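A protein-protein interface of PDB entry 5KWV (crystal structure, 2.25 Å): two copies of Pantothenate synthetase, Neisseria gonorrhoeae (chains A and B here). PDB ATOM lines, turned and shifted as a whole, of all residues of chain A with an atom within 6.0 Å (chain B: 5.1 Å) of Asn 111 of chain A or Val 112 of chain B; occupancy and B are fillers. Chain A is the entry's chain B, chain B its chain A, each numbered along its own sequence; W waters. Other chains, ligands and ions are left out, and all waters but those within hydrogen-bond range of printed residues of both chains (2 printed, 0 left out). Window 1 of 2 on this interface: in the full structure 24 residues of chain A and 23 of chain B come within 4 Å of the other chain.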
ATOM      1  N   LEU A  64       7.361   9.122  27.901  1.00  0.00           N
ATOM      2  CA  LEU A  64       8.105   9.263  26.650  1.00  0.00           C
ATOM      3  C   LEU A  64       9.622   9.286  26.819  1.00  0.00           C
ATOM      4  O   LEU A  64      10.330   9.274  25.806  1.00  0.00           O
ATOM      5  CB  LEU A  64       7.671  10.544  25.934  1.00  0.00           C
ATOM      6  CG  LEU A  64       6.572  10.490  24.868  1.00  0.00           C
ATOM      7  CD1 LEU A  64       5.329   9.735  25.323  1.00  0.00           C
ATOM      8  CD2 LEU A  64       6.248  11.927  24.451  1.00  0.00           C
ATOM      9  N   GLN A 108       2.091  10.824  21.108  1.00  0.00           N
ATOM     10  CA  GLN A 108       2.573  12.181  20.893  1.00  0.00           C
ATOM     11  C   GLN A 108       3.000  12.226  19.433  1.00  0.00           C
ATOM     12  O   GLN A 108       4.021  11.631  19.066  1.00  0.00           O
ATOM     13  CB  GLN A 108       3.743  12.495  21.824  1.00  0.00           C
ATOM     14  CG  GLN A 108       4.400  13.847  21.614  1.00  0.00           C
ATOM     15  CD  GLN A 108       3.552  14.975  22.149  1.00  0.00           C
ATOM     16  OE1 GLN A 108       2.628  14.741  22.934  1.00  0.00           O
ATOM     17  NE2 GLN A 108       3.859  16.214  21.737  1.00  0.00           N
ATOM     18  N   ARG A 109       2.202  12.900  18.591  1.00  0.00           N
ATOM     19  CA  ARG A 109       2.456  12.876  17.151  1.00  0.00           C
ATOM     20  C   ARG A 109       3.596  13.811  16.742  1.00  0.00           C
ATOM     21  O   ARG A 109       4.356  13.500  15.813  1.00  0.00           O
ATOM     22  CB  ARG A 109       1.183  13.251  16.376  1.00  0.00           C
ATOM     23  CG  ARG A 109      -0.005  12.296  16.489  1.00  0.00           C
ATOM     24  CD  ARG A 109      -1.314  13.014  16.017  1.00  0.00           C
ATOM     25  NE  ARG A 109      -1.619  14.176  16.858  1.00  0.00           N
ATOM     26  CZ  ARG A 109      -2.521  15.119  16.583  1.00  0.00           C
ATOM     27  NH1 ARG A 109      -3.243  15.067  15.471  1.00  0.00           N
ATOM     28  NH2 ARG A 109      -2.689  16.128  17.430  1.00  0.00           N
ATOM     29  N   TYR A 110       3.702  14.980  17.378  1.00  0.00           N
ATOM     30  CA  TYR A 110       4.703  15.993  17.046  1.00  0.00           C
ATOM     31  C   TYR A 110       5.739  16.011  18.159  1.00  0.00           C
ATOM     32  O   TYR A 110       5.412  16.324  19.309  1.00  0.00           O
ATOM     33  CB  TYR A 110       4.063  17.381  16.851  1.00  0.00           C
ATOM     34  CG  TYR A 110       3.176  17.370  15.625  1.00  0.00           C
ATOM     35  CD1 TYR A 110       3.648  17.843  14.397  1.00  0.00           C
ATOM     36  CD2 TYR A 110       1.892  16.831  15.674  1.00  0.00           C
ATOM     37  CE1 TYR A 110       2.861  17.794  13.256  1.00  0.00           C
ATOM     38  CE2 TYR A 110       1.103  16.748  14.539  1.00  0.00           C
ATOM     39  CZ  TYR A 110       1.591  17.240  13.335  1.00  0.00           C
ATOM     40  OH  TYR A 110       0.825  17.172  12.210  1.00  0.00           O
ATOM     41  N   ASN A 111       6.977  15.659  17.817  1.00  0.00           N
ATOM     42  CA  ASN A 111       8.058  15.552  18.779  1.00  0.00           C
ATOM     43  C   ASN A 111       9.144  16.548  18.416  1.00  0.00           C
ATOM     44  O   ASN A 111       9.312  16.904  17.252  1.00  0.00           O
ATOM     45  CB  ASN A 111       8.632  14.129  18.803  1.00  0.00           C
ATOM     46  CG  ASN A 111       7.578  13.102  19.188  1.00  0.00           C
ATOM     47  OD1 ASN A 111       7.358  12.842  20.366  1.00  0.00           O
ATOM     48  ND2 ASN A 111       6.871  12.558  18.179  1.00  0.00           N
ATOM     49  N   VAL A 112       9.857  17.034  19.422  1.00  0.00           N
ATOM     50  CA  VAL A 112      11.055  17.825  19.159  1.00  0.00           C
ATOM     51  C   VAL A 112      12.218  16.860  18.940  1.00  0.00           C
ATOM     52  O   VAL A 112      12.615  16.138  19.862  1.00  0.00           O
ATOM     53  CB  VAL A 112      11.327  18.805  20.311  1.00  0.00           C
ATOM     54  CG1 VAL A 112      12.638  19.556  20.097  1.00  0.00           C
ATOM     55  CG2 VAL A 112      10.156  19.778  20.454  1.00  0.00           C
ATOM     56  N   GLU A 113      12.783  16.858  17.727  1.00  0.00           N
ATOM     57  CA  GLU A 113      13.794  15.869  17.343  1.00  0.00           C
ATOM     58  C   GLU A 113      15.197  16.432  17.551  1.00  0.00           C
ATOM     59  O   GLU A 113      15.603  17.348  16.813  1.00  0.00           O
ATOM     60  CB  GLU A 113      13.599  15.444  15.884  1.00  0.00           C
ATOM     61  CG  GLU A 113      14.442  14.244  15.435  1.00  0.00           C
ATOM     62  CD  GLU A 113      14.045  12.970  16.144  1.00  0.00           C
ATOM     63  OE1 GLU A 113      12.899  12.883  16.620  1.00  0.00           O
ATOM     64  OE2 GLU A 113      14.889  12.066  16.247  1.00  0.00           O
ATOM     65  N   ARG A 131      14.888  12.621  22.919  1.00  0.00           N
ATOM     66  CA  ARG A 131      13.717  13.105  22.195  1.00  0.00           C
ATOM     67  C   ARG A 131      12.558  13.347  23.169  1.00  0.00           C
ATOM     68  O   ARG A 131      11.889  14.384  23.114  1.00  0.00           O
ATOM     69  CB  ARG A 131      13.320  12.109  21.101  1.00  0.00           C
ATOM     70  CG  ARG A 131      11.965  12.458  20.410  1.00  0.00           C
ATOM     71  CD  ARG A 131      11.428  11.327  19.499  1.00  0.00           C
ATOM     72  NE  ARG A 131      12.433  10.900  18.538  1.00  0.00           N
ATOM     73  CZ  ARG A 131      13.020   9.706  18.552  1.00  0.00           C
ATOM     74  NH1 ARG A 131      12.670   8.803  19.457  1.00  0.00           N
ATOM     75  NH2 ARG A 131      13.957   9.412  17.660  1.00  0.00           N
ATOM     76  N   THR A 135      10.883  17.012  24.006  1.00  0.00           N
ATOM     77  CA  THR A 135       9.471  17.193  23.716  1.00  0.00           C
ATOM     78  C   THR A 135       8.713  17.642  24.962  1.00  0.00           C
ATOM     79  O   THR A 135       8.002  18.649  24.925  1.00  0.00           O
ATOM     80  CB  THR A 135       8.897  15.893  23.155  1.00  0.00           C
ATOM     81  OG1 THR A 135       9.597  15.556  21.952  1.00  0.00           O
ATOM     82  CG2 THR A 135       7.398  16.042  22.847  1.00  0.00           C
ATOM     83  N   LEU A 169      14.673  26.836  18.748  1.00  0.00           N
ATOM     84  CA  LEU A 169      13.241  27.104  18.634  1.00  0.00           C
ATOM     85  C   LEU A 169      12.858  28.492  19.152  1.00  0.00           C
ATOM     86  O   LEU A 169      11.666  28.802  19.233  1.00  0.00           O
ATOM     87  CB  LEU A 169      12.440  26.029  19.375  1.00  0.00           C
ATOM     88  CG  LEU A 169      12.705  24.578  18.909  1.00  0.00           C
ATOM     89  CD1 LEU A 169      11.958  23.552  19.784  1.00  0.00           C
ATOM     90  CD2 LEU A 169      12.373  24.395  17.426  1.00  0.00           C
ATOM     91  N   TYR B 110      17.539  21.156  16.159  1.00  0.00           N
ATOM     92  CA  TYR B 110      16.312  20.709  16.810  1.00  0.00           C
ATOM     93  C   TYR B 110      15.135  21.065  15.902  1.00  0.00           C
ATOM     94  O   TYR B 110      14.868  22.245  15.652  1.00  0.00           O
ATOM     95  CB  TYR B 110      16.170  21.339  18.210  1.00  0.00           C
ATOM     96  CG  TYR B 110      17.261  20.843  19.137  1.00  0.00           C
ATOM     97  CD1 TYR B 110      17.049  19.761  19.998  1.00  0.00           C
ATOM     98  CD2 TYR B 110      18.540  21.402  19.085  1.00  0.00           C
ATOM     99  CE1 TYR B 110      18.089  19.268  20.808  1.00  0.00           C
ATOM    100  CE2 TYR B 110      19.583  20.923  19.885  1.00  0.00           C
ATOM    101  CZ  TYR B 110      19.357  19.867  20.734  1.00  0.00           C
ATOM    102  OH  TYR B 110      20.406  19.411  21.493  1.00  0.00           O
ATOM    103  N   ASN B 111      14.446  20.046  15.403  1.00  0.00           N
ATOM    104  CA  ASN B 111      13.348  20.240  14.471  1.00  0.00           C
ATOM    105  C   ASN B 111      12.053  19.724  15.078  1.00  0.00           C
ATOM    106  O   ASN B 111      12.050  18.742  15.827  1.00  0.00           O
ATOM    107  CB  ASN B 111      13.612  19.516  13.150  1.00  0.00           C
ATOM    108  CG  ASN B 111      14.813  20.067  12.434  1.00  0.00           C
ATOM    109  OD1 ASN B 111      14.691  21.037  11.683  1.00  0.00           O
ATOM    110  ND2 ASN B 111      15.990  19.460  12.666  1.00  0.00           N
ATOM    111  N   VAL B 112      10.944  20.355  14.718  1.00  0.00           N
ATOM    112  CA  VAL B 112       9.653  19.788  15.083  1.00  0.00           C
ATOM    113  C   VAL B 112       9.339  18.715  14.050  1.00  0.00           C
ATOM    114  O   VAL B 112       9.263  18.987  12.846  1.00  0.00           O
ATOM    115  CB  VAL B 112       8.556  20.862  15.161  1.00  0.00           C
ATOM    116  CG1 VAL B 112       7.185  20.201  15.484  1.00  0.00           C
ATOM    117  CG2 VAL B 112       8.915  21.917  16.242  1.00  0.00           C
ATOM    118  N   GLU B 113       9.252  17.482  14.508  1.00  0.00           N
ATOM    119  CA  GLU B 113       9.123  16.344  13.619  1.00  0.00           C
ATOM    120  C   GLU B 113       7.665  15.917  13.551  1.00  0.00           C
ATOM    121  O   GLU B 113       7.125  15.419  14.554  1.00  0.00           O
ATOM    122  CB  GLU B 113      10.005  15.194  14.106  1.00  0.00           C
ATOM    123  CG  GLU B 113      10.181  14.045  13.123  1.00  0.00           C
ATOM    124  CD  GLU B 113      10.987  14.416  11.882  1.00  0.00           C
ATOM    125  OE1 GLU B 113      10.836  13.732  10.845  1.00  0.00           O
ATOM    126  OE2 GLU B 113      11.777  15.373  11.934  1.00  0.00           O
ATOM    127  N   PRO B 114       6.984  16.113  12.426  1.00  0.00           N
ATOM    128  CA  PRO B 114       5.598  15.647  12.303  1.00  0.00           C
ATOM    129  C   PRO B 114       5.529  14.130  12.270  1.00  0.00           C
ATOM    130  O   PRO B 114       6.551  13.447  12.092  1.00  0.00           O
ATOM    131  CB  PRO B 114       5.138  16.252  10.964  1.00  0.00           C
ATOM    132  CG  PRO B 114       6.099  17.382  10.694  1.00  0.00           C
ATOM    133  CD  PRO B 114       7.411  16.895  11.255  1.00  0.00           C
ATOM    134  N   ARG B 131       8.312  19.042   7.763  1.00  0.00           N
ATOM    135  CA  ARG B 131       9.201  19.235   8.908  1.00  0.00           C
ATOM    136  C   ARG B 131       9.684  20.682   8.973  1.00  0.00           C
ATOM    137  O   ARG B 131       9.620  21.325  10.030  1.00  0.00           O
ATOM    138  CB  ARG B 131      10.402  18.268   8.833  1.00  0.00           C
ATOM    139  CG  ARG B 131      11.536  18.618   9.821  1.00  0.00           C
ATOM    140  CD  ARG B 131      12.869  17.800   9.568  1.00  0.00           C
ATOM    141  NE  ARG B 131      12.621  16.366   9.567  1.00  0.00           N
ATOM    142  CZ  ARG B 131      12.704  15.589   8.485  1.00  0.00           C
ATOM    143  NH1 ARG B 131      13.068  16.102   7.313  1.00  0.00           N
ATOM    144  NH2 ARG B 131      12.444  14.288   8.573  1.00  0.00           N
ATOM    145  N   ALA B 134       6.768  22.953   9.973  1.00  0.00           N
ATOM    146  CA  ALA B 134       6.418  22.802  11.380  1.00  0.00           C
ATOM    147  C   ALA B 134       7.450  23.489  12.244  1.00  0.00           C
ATOM    148  O   ALA B 134       7.099  24.172  13.213  1.00  0.00           O
ATOM    149  CB  ALA B 134       6.317  21.322  11.751  1.00  0.00           C
ATOM    150  N   THR B 135       8.732  23.372  11.860  1.00  0.00           N
ATOM    151  CA  THR B 135       9.814  23.943  12.656  1.00  0.00           C
ATOM    152  C   THR B 135       9.789  25.463  12.604  1.00  0.00           C
ATOM    153  O   THR B 135       9.889  26.136  13.640  1.00  0.00           O
ATOM    154  CB  THR B 135      11.161  23.396  12.168  1.00  0.00           C
ATOM    155  OG1 THR B 135      11.163  21.963  12.296  1.00  0.00           O
ATOM    156  CG2 THR B 135      12.303  23.983  12.988  1.00  0.00           C
ATOM    157  N   SER B 138       6.823  26.918  14.578  1.00  0.00           N
ATOM    158  CA  SER B 138       7.073  26.901  16.018  1.00  0.00           C
ATOM    159  C   SER B 138       8.002  28.046  16.431  1.00  0.00           C
ATOM    160  O   SER B 138       7.747  28.747  17.427  1.00  0.00           O
ATOM    161  CB  SER B 138       7.659  25.549  16.417  1.00  0.00           C
ATOM    162  OG  SER B 138       6.757  24.496  16.088  1.00  0.00           O
ATOM    163  N   LEU B 165       0.729  20.329  15.629  1.00  0.00           N
ATOM    164  CA  LEU B 165       1.838  20.766  16.489  1.00  0.00           C
ATOM    165  C   LEU B 165       1.360  21.726  17.582  1.00  0.00           C
ATOM    166  O   LEU B 165       1.897  21.716  18.695  1.00  0.00           O
ATOM    167  CB  LEU B 165       2.952  21.411  15.656  1.00  0.00           C
ATOM    168  CG  LEU B 165       2.766  22.810  15.038  1.00  0.00           C
ATOM    169  CD1 LEU B 165       3.073  23.944  16.028  1.00  0.00           C
ATOM    170  CD2 LEU B 165       3.649  22.969  13.793  1.00  0.00           C
ATOM    171  N   LEU B 169       2.285  20.366  21.227  1.00  0.00           N
ATOM    172  CA  LEU B 169       3.300  21.127  21.953  1.00  0.00           C
ATOM    173  C   LEU B 169       2.684  22.212  22.844  1.00  0.00           C
ATOM    174  O   LEU B 169       3.412  23.064  23.361  1.00  0.00           O
ATOM    175  CB  LEU B 169       4.327  21.715  20.971  1.00  0.00           C
ATOM    176  CG  LEU B 169       5.078  20.661  20.093  1.00  0.00           C
ATOM    177  CD1 LEU B 169       5.980  21.301  19.076  1.00  0.00           C
ATOM    178  CD2 LEU B 169       5.929  19.715  20.966  1.00  0.00           C
HETATM  179  O   HOH W   1      16.346  17.038  14.086  1.00  0.00           O
HETATM  180  O   HOH W   2       7.496  12.847  15.562  1.00  0.00           O
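Hydrophobic or aromatic side chains of chain B within 4 Å of the printed part of chain A: Pro 114, Leu 165 and Leu 169. Of the 10 printed residues of chain A, 6 touch a printed residue of chain B. Along chain A the printed residues that touch a printed residue of chain B span positions 109 to 169. Among the printed residues, 13 pairs touch across the chains.
Arg 109 of chain A touches Glu 113 of chain B (O to O, 3.6 Å). O of Arg 109 of chain A touches C of Pro 114 of chain B (3.8 Å). Tyr 110 of chain A touches Glu 113 of chain B (CA to O, 3.5 Å). Leu 165 of chain B touches Tyr 110 of chain A (N to CD2, 3.7 Å). Tyr 110 of chain A touches Leu 169 of chain B. Asn 111 of chain A touches Asn 111 of chain B. Asn 111 of chain A touches Val 112 of chain B. O of Asn 111 of chain B touches CA of Val 112 of chain A, at 3.6 Å. Tyr 110 of chain B touches Glu 113 of chain A. Tyr 110 of chain B touches Leu 169 of chain A (O to CD2, 3.7 Å).
OE1 of Glu 113 of chain A lies within salt-bridge range of NE of Arg 131 of chain A (2.8 Å). The guanidinium group of Arg 131 of chain B lies within salt-bridge range of the side-chain carboxylate of Glu 113 of chain B, at 2.7 Å. OG1 of Thr 135 of chain B lies within hydrogen-bond range of N of Val 112 of chain B (2.9 Å). The side-chain amide nitrogen of Asn 111 of chain A sits at hydrogen-bond distance from the backbone carbonyl oxygen of Gln 108 of chain A (3.1 Å). O of Tyr 110 of chain A is in hydrogen-bond range of NE2 of Gln 108 of chain A, at 2.9 Å. N of Val 112 of chain A sits at hydrogen-bond distance from OG1 of Thr 135 of chain A (2.9 Å).
Printed residues of chain B within 4 Å of Tyr 110 of chain A: Glu 113, Pro 114, Leu 165 and Leu 169. Asn 111 of chain A touches just these residues of chain B: Asn 111 (3.6 Å), Val 112 (3.6 Å) and Glu 113 (2.8 Å). Val 112 of chain B touches one residue of chain A. Printed residues of chain A within 4 Å of Leu 169 of chain B: Tyr 110 (3.8 Å). The nearest printed residue of chain A that does not touch Glu 113 of chain B is Glu 113 of chain A (4.02 Å).
Tyr 110 of chain A touches Leu 169 of chain B, and with the chains exchanged Leu 169 of chain A touches Tyr 110 of chain B. Asn 111 of chain A touches its own counterpart, Asn 111 of chain B. Asn 111 of chain A touches Val 112 of chain B, and with the chains exchanged Val 112 of chain A touches Asn 111 of chain B. Asn 111 of chain A touches Glu 113 of chain B, and with the chains exchanged Glu 113 of chain A touches Asn 111 of chain B. 7 positions are printed for both chains. Of the 13 pairs that touch across the chains among the printed residues, 9 have their exchanged pair printed and touching as well.
Water W2 lies within hydrogen-bond range of the side-chain amide nitrogen (ND2) of Asn 111 of chain A (2.7 Å), the backbone carbonyl oxygen (O) of Glu 113 of chain B (2.8 Å) and the backbone carbonyl oxygen (O) of Arg 109 of chain A (3.2 Å). Water W1 lies within hydrogen-bond range of the side-chain amide nitrogen of Asn 111 of chain B (2.8 Å) and the backbone carbonyl oxygen of Glu 113 of chain A (2.8 Å).
The backbone NH (N) of Glu 113 of chain B lies within hydrogen-bond range of the backbone carbonyl oxygen (O) of Asn 111 of chain A, at 2.8 Å. The backbone NH of Glu 113 of chain A lies within hydrogen-bond range of the backbone carbonyl oxygen of Asn 111 of chain B (2.8 Å).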
